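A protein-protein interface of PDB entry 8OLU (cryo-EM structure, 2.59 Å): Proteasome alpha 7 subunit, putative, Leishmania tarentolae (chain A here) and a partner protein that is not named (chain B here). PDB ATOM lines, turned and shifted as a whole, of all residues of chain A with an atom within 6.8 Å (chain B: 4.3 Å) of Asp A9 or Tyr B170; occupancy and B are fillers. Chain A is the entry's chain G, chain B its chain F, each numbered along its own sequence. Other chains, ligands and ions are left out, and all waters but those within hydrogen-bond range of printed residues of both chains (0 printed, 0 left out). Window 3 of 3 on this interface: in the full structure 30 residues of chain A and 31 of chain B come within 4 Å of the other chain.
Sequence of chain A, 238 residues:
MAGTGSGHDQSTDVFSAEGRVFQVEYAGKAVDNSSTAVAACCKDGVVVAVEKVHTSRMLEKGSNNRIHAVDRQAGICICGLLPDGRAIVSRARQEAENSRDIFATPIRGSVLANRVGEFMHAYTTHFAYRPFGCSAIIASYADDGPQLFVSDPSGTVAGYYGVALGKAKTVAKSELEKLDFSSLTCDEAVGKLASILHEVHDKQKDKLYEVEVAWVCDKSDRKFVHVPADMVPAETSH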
ATOM      1  N   GLY A   7     -10.254  31.195   5.953  1.00  0.00           N
ATOM      2  CA  GLY A   7      -9.002  30.840   5.244  1.00  0.00           C
ATOM      3  C   GLY A   7      -8.080  29.924   6.060  1.00  0.00           C
ATOM      4  O   GLY A   7      -7.019  29.520   5.578  1.00  0.00           O
ATOM      5  N   HIS A   8      -8.520  29.569   7.274  1.00  0.00           N
ATOM      6  CA  HIS A   8      -7.789  28.699   8.188  1.00  0.00           C
ATOM      7  C   HIS A   8      -7.851  27.222   7.779  1.00  0.00           C
ATOM      8  O   HIS A   8      -7.242  26.410   8.473  1.00  0.00           O
ATOM      9  CB  HIS A   8      -8.338  28.874   9.628  1.00  0.00           C
ATOM     10  CG  HIS A   8      -9.834  28.741   9.769  1.00  0.00           C
ATOM     11  ND1 HIS A   8     -10.752  29.550   9.118  1.00  0.00           N
ATOM     12  CD2 HIS A   8     -10.564  27.838  10.495  1.00  0.00           C
ATOM     13  CE1 HIS A   8     -11.989  29.158   9.423  1.00  0.00           C
ATOM     14  NE2 HIS A   8     -11.895  28.091  10.278  1.00  0.00           N
ATOM     15  N   ASP A   9      -8.625  26.851   6.727  1.00  0.00           N
ATOM     16  CA  ASP A   9      -9.054  25.468   6.571  1.00  0.00           C
ATOM     17  C   ASP A   9      -8.946  24.972   5.143  1.00  0.00           C
ATOM     18  O   ASP A   9      -9.547  23.983   4.757  1.00  0.00           O
ATOM     19  CB  ASP A   9     -10.478  25.247   7.081  1.00  0.00           C
ATOM     20  CG  ASP A   9     -11.588  25.889   6.269  1.00  0.00           C
ATOM     21  OD1 ASP A   9     -12.735  25.658   6.659  1.00  0.00           O
ATOM     22  OD2 ASP A   9     -11.309  26.600   5.241  1.00  0.00           O
ATOM     23  N   GLN A  10      -8.145  25.635   4.356  1.00  0.00           N
ATOM     24  CA  GLN A  10      -8.112  25.367   2.947  1.00  0.00           C
ATOM     25  C   GLN A  10      -6.923  24.475   2.601  1.00  0.00           C
ATOM     26  O   GLN A  10      -6.875  23.854   1.531  1.00  0.00           O
ATOM     27  CB  GLN A  10      -7.949  26.710   2.278  1.00  0.00           C
ATOM     28  CG  GLN A  10      -9.154  27.607   2.450  1.00  0.00           C
ATOM     29  CD  GLN A  10     -10.197  27.306   1.413  1.00  0.00           C
ATOM     30  OE1 GLN A  10      -9.934  27.406   0.210  1.00  0.00           O
ATOM     31  NE2 GLN A  10     -11.362  26.901   1.896  1.00  0.00           N
ATOM     32  N   SER A  11      -5.922  24.477   3.480  1.00  0.00           N
ATOM     33  CA  SER A  11      -4.745  23.702   3.220  1.00  0.00           C
ATOM     34  C   SER A  11      -4.347  22.975   4.480  1.00  0.00           C
ATOM     35  O   SER A  11      -4.606  23.400   5.606  1.00  0.00           O
ATOM     36  CB  SER A  11      -3.668  24.604   2.739  1.00  0.00           C
ATOM     37  OG  SER A  11      -2.672  23.882   1.994  1.00  0.00           O
ATOM     38  N   THR A  12      -3.822  21.786   4.278  1.00  0.00           N
ATOM     39  CA  THR A  12      -3.424  21.009   5.425  1.00  0.00           C
ATOM     40  C   THR A  12      -2.138  21.565   6.004  1.00  0.00           C
ATOM     41  O   THR A  12      -1.817  21.197   7.112  1.00  0.00           O
ATOM     42  CB  THR A  12      -3.178  19.559   5.079  1.00  0.00           C
ATOM     43  OG1 THR A  12      -2.862  18.846   6.270  1.00  0.00           O
ATOM     44  CG2 THR A  12      -1.998  19.405   4.146  1.00  0.00           C
ATOM     45  N   VAL A  14      -1.680  24.168   7.444  1.00  0.00           N
ATOM     46  CA  VAL A  14      -1.993  25.293   8.285  1.00  0.00           C
ATOM     47  C   VAL A  14      -2.659  24.840   9.551  1.00  0.00           C
ATOM     48  O   VAL A  14      -3.654  24.134   9.501  1.00  0.00           O
ATOM     49  CB  VAL A  14      -2.947  26.188   7.503  1.00  0.00           C
ATOM     50  CG1 VAL A  14      -3.610  27.201   8.400  1.00  0.00           C
ATOM     51  CG2 VAL A  14      -2.147  26.877   6.413  1.00  0.00           C
ATOM     52  N   VAL A  21      -5.754  20.875  12.588  1.00  0.00           N
ATOM     53  CA  VAL A  21      -5.569  20.975  11.179  1.00  0.00           C
ATOM     54  C   VAL A  21      -6.860  20.558  10.516  1.00  0.00           C
ATOM     55  O   VAL A  21      -7.125  19.393  10.334  1.00  0.00           O
ATOM     56  CB  VAL A  21      -4.485  20.016  10.716  1.00  0.00           C
ATOM     57  CG1 VAL A  21      -4.274  20.116   9.229  1.00  0.00           C
ATOM     58  CG2 VAL A  21      -3.179  20.167  11.490  1.00  0.00           C
ATOM     59  N   PHE A  22      -7.602  21.519  10.026  1.00  0.00           N
ATOM     60  CA  PHE A  22      -8.925  21.231   9.563  1.00  0.00           C
ATOM     61  C   PHE A  22      -8.943  20.339   8.351  1.00  0.00           C
ATOM     62  O   PHE A  22      -9.762  19.461   8.251  1.00  0.00           O
ATOM     63  CB  PHE A  22      -9.606  22.551   9.301  1.00  0.00           C
ATOM     64  CG  PHE A  22     -10.271  23.092  10.528  1.00  0.00           C
ATOM     65  CD1 PHE A  22     -11.464  22.557  10.963  1.00  0.00           C
ATOM     66  CD2 PHE A  22      -9.704  24.102  11.259  1.00  0.00           C
ATOM     67  CE1 PHE A  22     -12.090  23.046  12.098  1.00  0.00           C
ATOM     68  CE2 PHE A  22     -10.356  24.621  12.365  1.00  0.00           C
ATOM     69  CZ  PHE A  22     -11.528  24.077  12.795  1.00  0.00           C
ATOM     70  N   GLN A  23      -8.086  20.553   7.381  1.00  0.00           N
ATOM     71  CA  GLN A  23      -8.152  19.690   6.226  1.00  0.00           C
ATOM     72  C   GLN A  23      -7.992  18.232   6.597  1.00  0.00           C
ATOM     73  O   GLN A  23      -8.466  17.352   5.890  1.00  0.00           O
ATOM     74  CB  GLN A  23      -7.067  20.033   5.247  1.00  0.00           C
ATOM     75  CG  GLN A  23      -7.474  21.262   4.443  1.00  0.00           C
ATOM     76  CD  GLN A  23      -8.510  20.927   3.443  1.00  0.00           C
ATOM     77  OE1 GLN A  23      -8.266  20.069   2.606  1.00  0.00           O
ATOM     78  NE2 GLN A  23      -9.632  21.616   3.512  1.00  0.00           N
ATOM     79  N   TYR A  26     -11.516  17.251   8.005  1.00  0.00           N
ATOM     80  CA  TYR A  26     -12.398  17.104   6.857  1.00  0.00           C
ATOM     81  C   TYR A  26     -12.149  15.773   6.142  1.00  0.00           C
ATOM     82  O   TYR A  26     -13.069  15.020   5.908  1.00  0.00           O
ATOM     83  CB  TYR A  26     -12.223  18.308   5.950  1.00  0.00           C
ATOM     84  CG  TYR A  26     -12.616  19.637   6.551  1.00  0.00           C
ATOM     85  CD1 TYR A  26     -13.356  19.716   7.702  1.00  0.00           C
ATOM     86  CD2 TYR A  26     -12.276  20.829   5.917  1.00  0.00           C
ATOM     87  CE1 TYR A  26     -13.717  20.940   8.238  1.00  0.00           C
ATOM     88  CE2 TYR A  26     -12.599  22.057   6.466  1.00  0.00           C
ATOM     89  CZ  TYR A  26     -13.357  22.116   7.615  1.00  0.00           C
ATOM     90  OH  TYR A  26     -13.751  23.326   8.164  1.00  0.00           O
ATOM     91  N   ASN B 168     -19.131  28.879  -2.660  1.00  0.00           N
ATOM     92  CA  ASN B 168     -18.422  27.631  -2.258  1.00  0.00           C
ATOM     93  C   ASN B 168     -16.920  27.908  -2.171  1.00  0.00           C
ATOM     94  O   ASN B 168     -16.257  28.124  -3.178  1.00  0.00           O
ATOM     95  CB  ASN B 168     -18.720  26.468  -3.215  1.00  0.00           C
ATOM     96  CG  ASN B 168     -18.330  25.122  -2.636  1.00  0.00           C
ATOM     97  OD1 ASN B 168     -17.215  24.968  -2.129  1.00  0.00           O
ATOM     98  ND2 ASN B 168     -19.249  24.162  -2.686  1.00  0.00           N
ATOM     99  N   GLU B 169     -16.367  27.902  -0.958  1.00  0.00           N
ATOM    100  CA  GLU B 169     -15.005  28.375  -0.798  1.00  0.00           C
ATOM    101  C   GLU B 169     -14.023  27.226  -1.099  1.00  0.00           C
ATOM    102  O   GLU B 169     -12.819  27.447  -1.177  1.00  0.00           O
ATOM    103  CB  GLU B 169     -14.884  29.062   0.571  1.00  0.00           C
ATOM    104  CG  GLU B 169     -13.743  30.094   0.625  1.00  0.00           C
ATOM    105  CD  GLU B 169     -13.980  31.388   1.406  1.00  0.00           C
ATOM    106  OE1 GLU B 169     -14.265  31.316   2.630  1.00  0.00           O
ATOM    107  OE2 GLU B 169     -13.859  32.476   0.797  1.00  0.00           O
ATOM    108  N   TYR B 170     -14.558  26.022  -1.385  1.00  0.00           N
ATOM    109  CA  TYR B 170     -13.823  24.772  -1.280  1.00  0.00           C
ATOM    110  C   TYR B 170     -13.743  24.013  -2.599  1.00  0.00           C
ATOM    111  O   TYR B 170     -13.273  22.878  -2.636  1.00  0.00           O
ATOM    112  CB  TYR B 170     -14.575  23.881  -0.298  1.00  0.00           C
ATOM    113  CG  TYR B 170     -14.586  24.427   1.098  1.00  0.00           C
ATOM    114  CD1 TYR B 170     -13.470  24.316   1.903  1.00  0.00           C
ATOM    115  CD2 TYR B 170     -15.698  25.079   1.613  1.00  0.00           C
ATOM    116  CE1 TYR B 170     -13.449  24.841   3.185  1.00  0.00           C
ATOM    117  CE2 TYR B 170     -15.699  25.584   2.908  1.00  0.00           C
ATOM    118  CZ  TYR B 170     -14.563  25.479   3.699  1.00  0.00           C
ATOM    119  OH  TYR B 170     -14.546  25.954   4.987  1.00  0.00           O
ATOM    120  N   ASP B 171     -14.229  24.623  -3.682  1.00  0.00           N
ATOM    121  CA  ASP B 171     -14.470  23.911  -4.923  1.00  0.00           C
ATOM    122  C   ASP B 171     -13.508  24.355  -6.008  1.00  0.00           C
ATOM    123  O   ASP B 171     -13.752  24.088  -7.172  1.00  0.00           O
ATOM    124  CB  ASP B 171     -15.909  24.098  -5.399  1.00  0.00           C
ATOM    125  CG  ASP B 171     -16.153  25.423  -6.090  1.00  0.00           C
ATOM    126  OD1 ASP B 171     -15.302  26.320  -5.917  1.00  0.00           O
ATOM    127  OD2 ASP B 171     -17.180  25.533  -6.844  1.00  0.00           O
ATOM    128  N   SER B 172     -12.390  24.964  -5.637  1.00  0.00           N
ATOM    129  CA  SER B 172     -11.537  25.594  -6.625  1.00  0.00           C
ATOM    130  C   SER B 172     -10.240  24.826  -6.781  1.00  0.00           C
ATOM    131  O   SER B 172      -9.493  25.119  -7.702  1.00  0.00           O
ATOM    132  CB  SER B 172     -11.291  27.045  -6.280  1.00  0.00           C
ATOM    133  OG  SER B 172     -12.341  27.864  -6.826  1.00  0.00           O
ATOM    134  N   THR B 176      -8.428  20.329  -1.910  1.00  0.00           N
ATOM    135  CA  THR B 176      -9.114  20.898  -0.781  1.00  0.00           C
ATOM    136  C   THR B 176     -10.331  20.095  -0.437  1.00  0.00           C
ATOM    137  O   THR B 176     -11.230  19.950  -1.248  1.00  0.00           O
ATOM    138  CB  THR B 176      -9.444  22.345  -1.059  1.00  0.00           C
ATOM    139  OG1 THR B 176      -8.150  22.957  -1.077  1.00  0.00           O
ATOM    140  CG2 THR B 176     -10.295  22.885   0.060  1.00  0.00           C
ATOM    141  N   TRP B 177     -10.337  19.547   0.750  1.00  0.00           N
ATOM    142  CA  TRP B 177     -11.520  18.865   1.202  1.00  0.00           C
ATOM    143  C   TRP B 177     -12.501  19.921   1.545  1.00  0.00           C
ATOM    144  O   TRP B 177     -12.070  20.976   1.916  1.00  0.00           O
ATOM    145  CB  TRP B 177     -11.229  18.049   2.429  1.00  0.00           C
ATOM    146  CG  TRP B 177     -10.407  16.863   2.102  1.00  0.00           C
ATOM    147  CD1 TRP B 177      -9.068  16.717   2.234  1.00  0.00           C
ATOM    148  CD2 TRP B 177     -10.912  15.602   1.694  1.00  0.00           C
ATOM    149  NE1 TRP B 177      -8.684  15.442   1.902  1.00  0.00           N
ATOM    150  CE2 TRP B 177      -9.807  14.731   1.598  1.00  0.00           C
ATOM    151  CE3 TRP B 177     -12.198  15.130   1.470  1.00  0.00           C
ATOM    152  CZ2 TRP B 177      -9.945  13.420   1.174  1.00  0.00           C
ATOM    153  CZ3 TRP B 177     -12.340  13.842   1.042  1.00  0.00           C
ATOM    154  CH2 TRP B 177     -11.235  12.996   0.885  1.00  0.00           C
ATOM    155  N   SER B 178     -13.763  19.596   1.413  1.00  0.00           N
ATOM    156  CA  SER B 178     -14.787  20.467   1.920  1.00  0.00           C
ATOM    157  C   SER B 178     -15.052  20.025   3.333  1.00  0.00           C
ATOM    158  O   SER B 178     -14.739  18.904   3.672  1.00  0.00           O
ATOM    159  CB  SER B 178     -16.057  20.410   1.112  1.00  0.00           C
ATOM    160  OG  SER B 178     -16.798  19.245   1.443  1.00  0.00           O
ATOM    161  N   PRO B 179     -15.682  20.836   4.174  1.00  0.00           N
ATOM    162  CA  PRO B 179     -16.027  20.410   5.524  1.00  0.00           C
ATOM    163  C   PRO B 179     -16.968  19.242   5.708  1.00  0.00           C
ATOM    164  O   PRO B 179     -17.114  18.761   6.822  1.00  0.00           O
ATOM    165  CB  PRO B 179     -16.776  21.619   6.082  1.00  0.00           C
ATOM    166  CG  PRO B 179     -16.106  22.759   5.344  1.00  0.00           C
ATOM    167  CD  PRO B 179     -15.957  22.243   3.921  1.00  0.00           C
ATOM    168  N   PHE B 184     -14.901  18.622  -4.308  1.00  0.00           N
ATOM    169  CA  PHE B 184     -15.687  19.147  -5.403  1.00  0.00           C
ATOM    170  C   PHE B 184     -14.967  19.089  -6.743  1.00  0.00           C
ATOM    171  O   PHE B 184     -15.617  18.781  -7.737  1.00  0.00           O
ATOM    172  CB  PHE B 184     -16.110  20.568  -5.117  1.00  0.00           C
ATOM    173  CG  PHE B 184     -17.168  20.619  -4.076  1.00  0.00           C
ATOM    174  CD1 PHE B 184     -18.442  20.180  -4.357  1.00  0.00           C
ATOM    175  CD2 PHE B 184     -16.890  21.084  -2.814  1.00  0.00           C
ATOM    176  CE1 PHE B 184     -19.434  20.228  -3.395  1.00  0.00           C
ATOM    177  CE2 PHE B 184     -17.888  21.117  -1.854  1.00  0.00           C
ATOM    178  CZ  PHE B 184     -19.151  20.671  -2.137  1.00  0.00           C
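N of Trp B177 is in hydrogen-bond range of OE1 of Gln A23 (2.8 Å).
The backbone carbonyl oxygen (O) of Glu B169 sits close to the side-chain amide oxygen (OE1) of Gln A10.
O of Gln A10 is in hydrogen-bond range of OG1 of Thr B176.
The side-chain hydroxyl (OH) of Tyr B170 sits at hydrogen-bond distance from the side-chain carboxylate (OD1) of Asp A9 (2.5 Å).
Of chain B, only Tyr B170 comes within 4 Å of Asp A9.
Tyr B170 touches just these residues of chain A: Asp A9 (2.5 Å) and Gln A10 (3.2 Å).
Printed residues of chain A within 4 Å of Glu B169: Gln A10.
Printed residues of chain A within 4 Å of Pro B179: Tyr A26.
Of the printed residues of chain B, Tyr A26 touches Trp B177, Ser B178 and Pro B179.
Printed residues of chain B within 4 Å of Gln A10: Glu B169, Tyr B170 and Thr B176.
The nearest printed residue of chain B that does not touch Asp A9 is Pro B179 (4.6 Å).
The nearest residue of chain A that does not touch Tyr B170 is Tyr A26 (4.2 Å).
The nearest printed residue of chain A that does not touch Thr B176 is Asp A9 (4.9 Å).
Among the printed residues, merely in contact across the chains: Gln A10 with Tyr B170, Gln A23 with Thr B176, Tyr A26 with Trp B177, Tyr A26 with Ser B178 and Tyr A26 with Pro B179.
Of the 11 printed residues of chain A, 4 touch a printed residue of chain B.
Of the 10 printed residues of chain B, 6 touch a printed residue of chain A.
Hydrophobic or aromatic side chains of chain B within 4 Å of the printed part of chain A: Tyr B170, Trp B177 and Pro B179.
Among the printed residues, no Asp or Glu carboxylate lies within 4 Å of a Lys or Arg side-chain nitrogen of the other chain.
NE2 of Gln A10 sits at hydrogen-bond distance from OD2 of Asp A9.
The side-chain amide oxygen of Asn B168 sits at hydrogen-bond distance from the backbone NH of Tyr B170.
The side-chain hydroxyl (OH) of Tyr A26 lies within hydrogen-bond range of the side-chain carboxylate (OD1) of Asp A9, at 3.0 Å.
O of Asp A9 sits at hydrogen-bond distance from NE2 of Gln A23 (2.7 Å).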
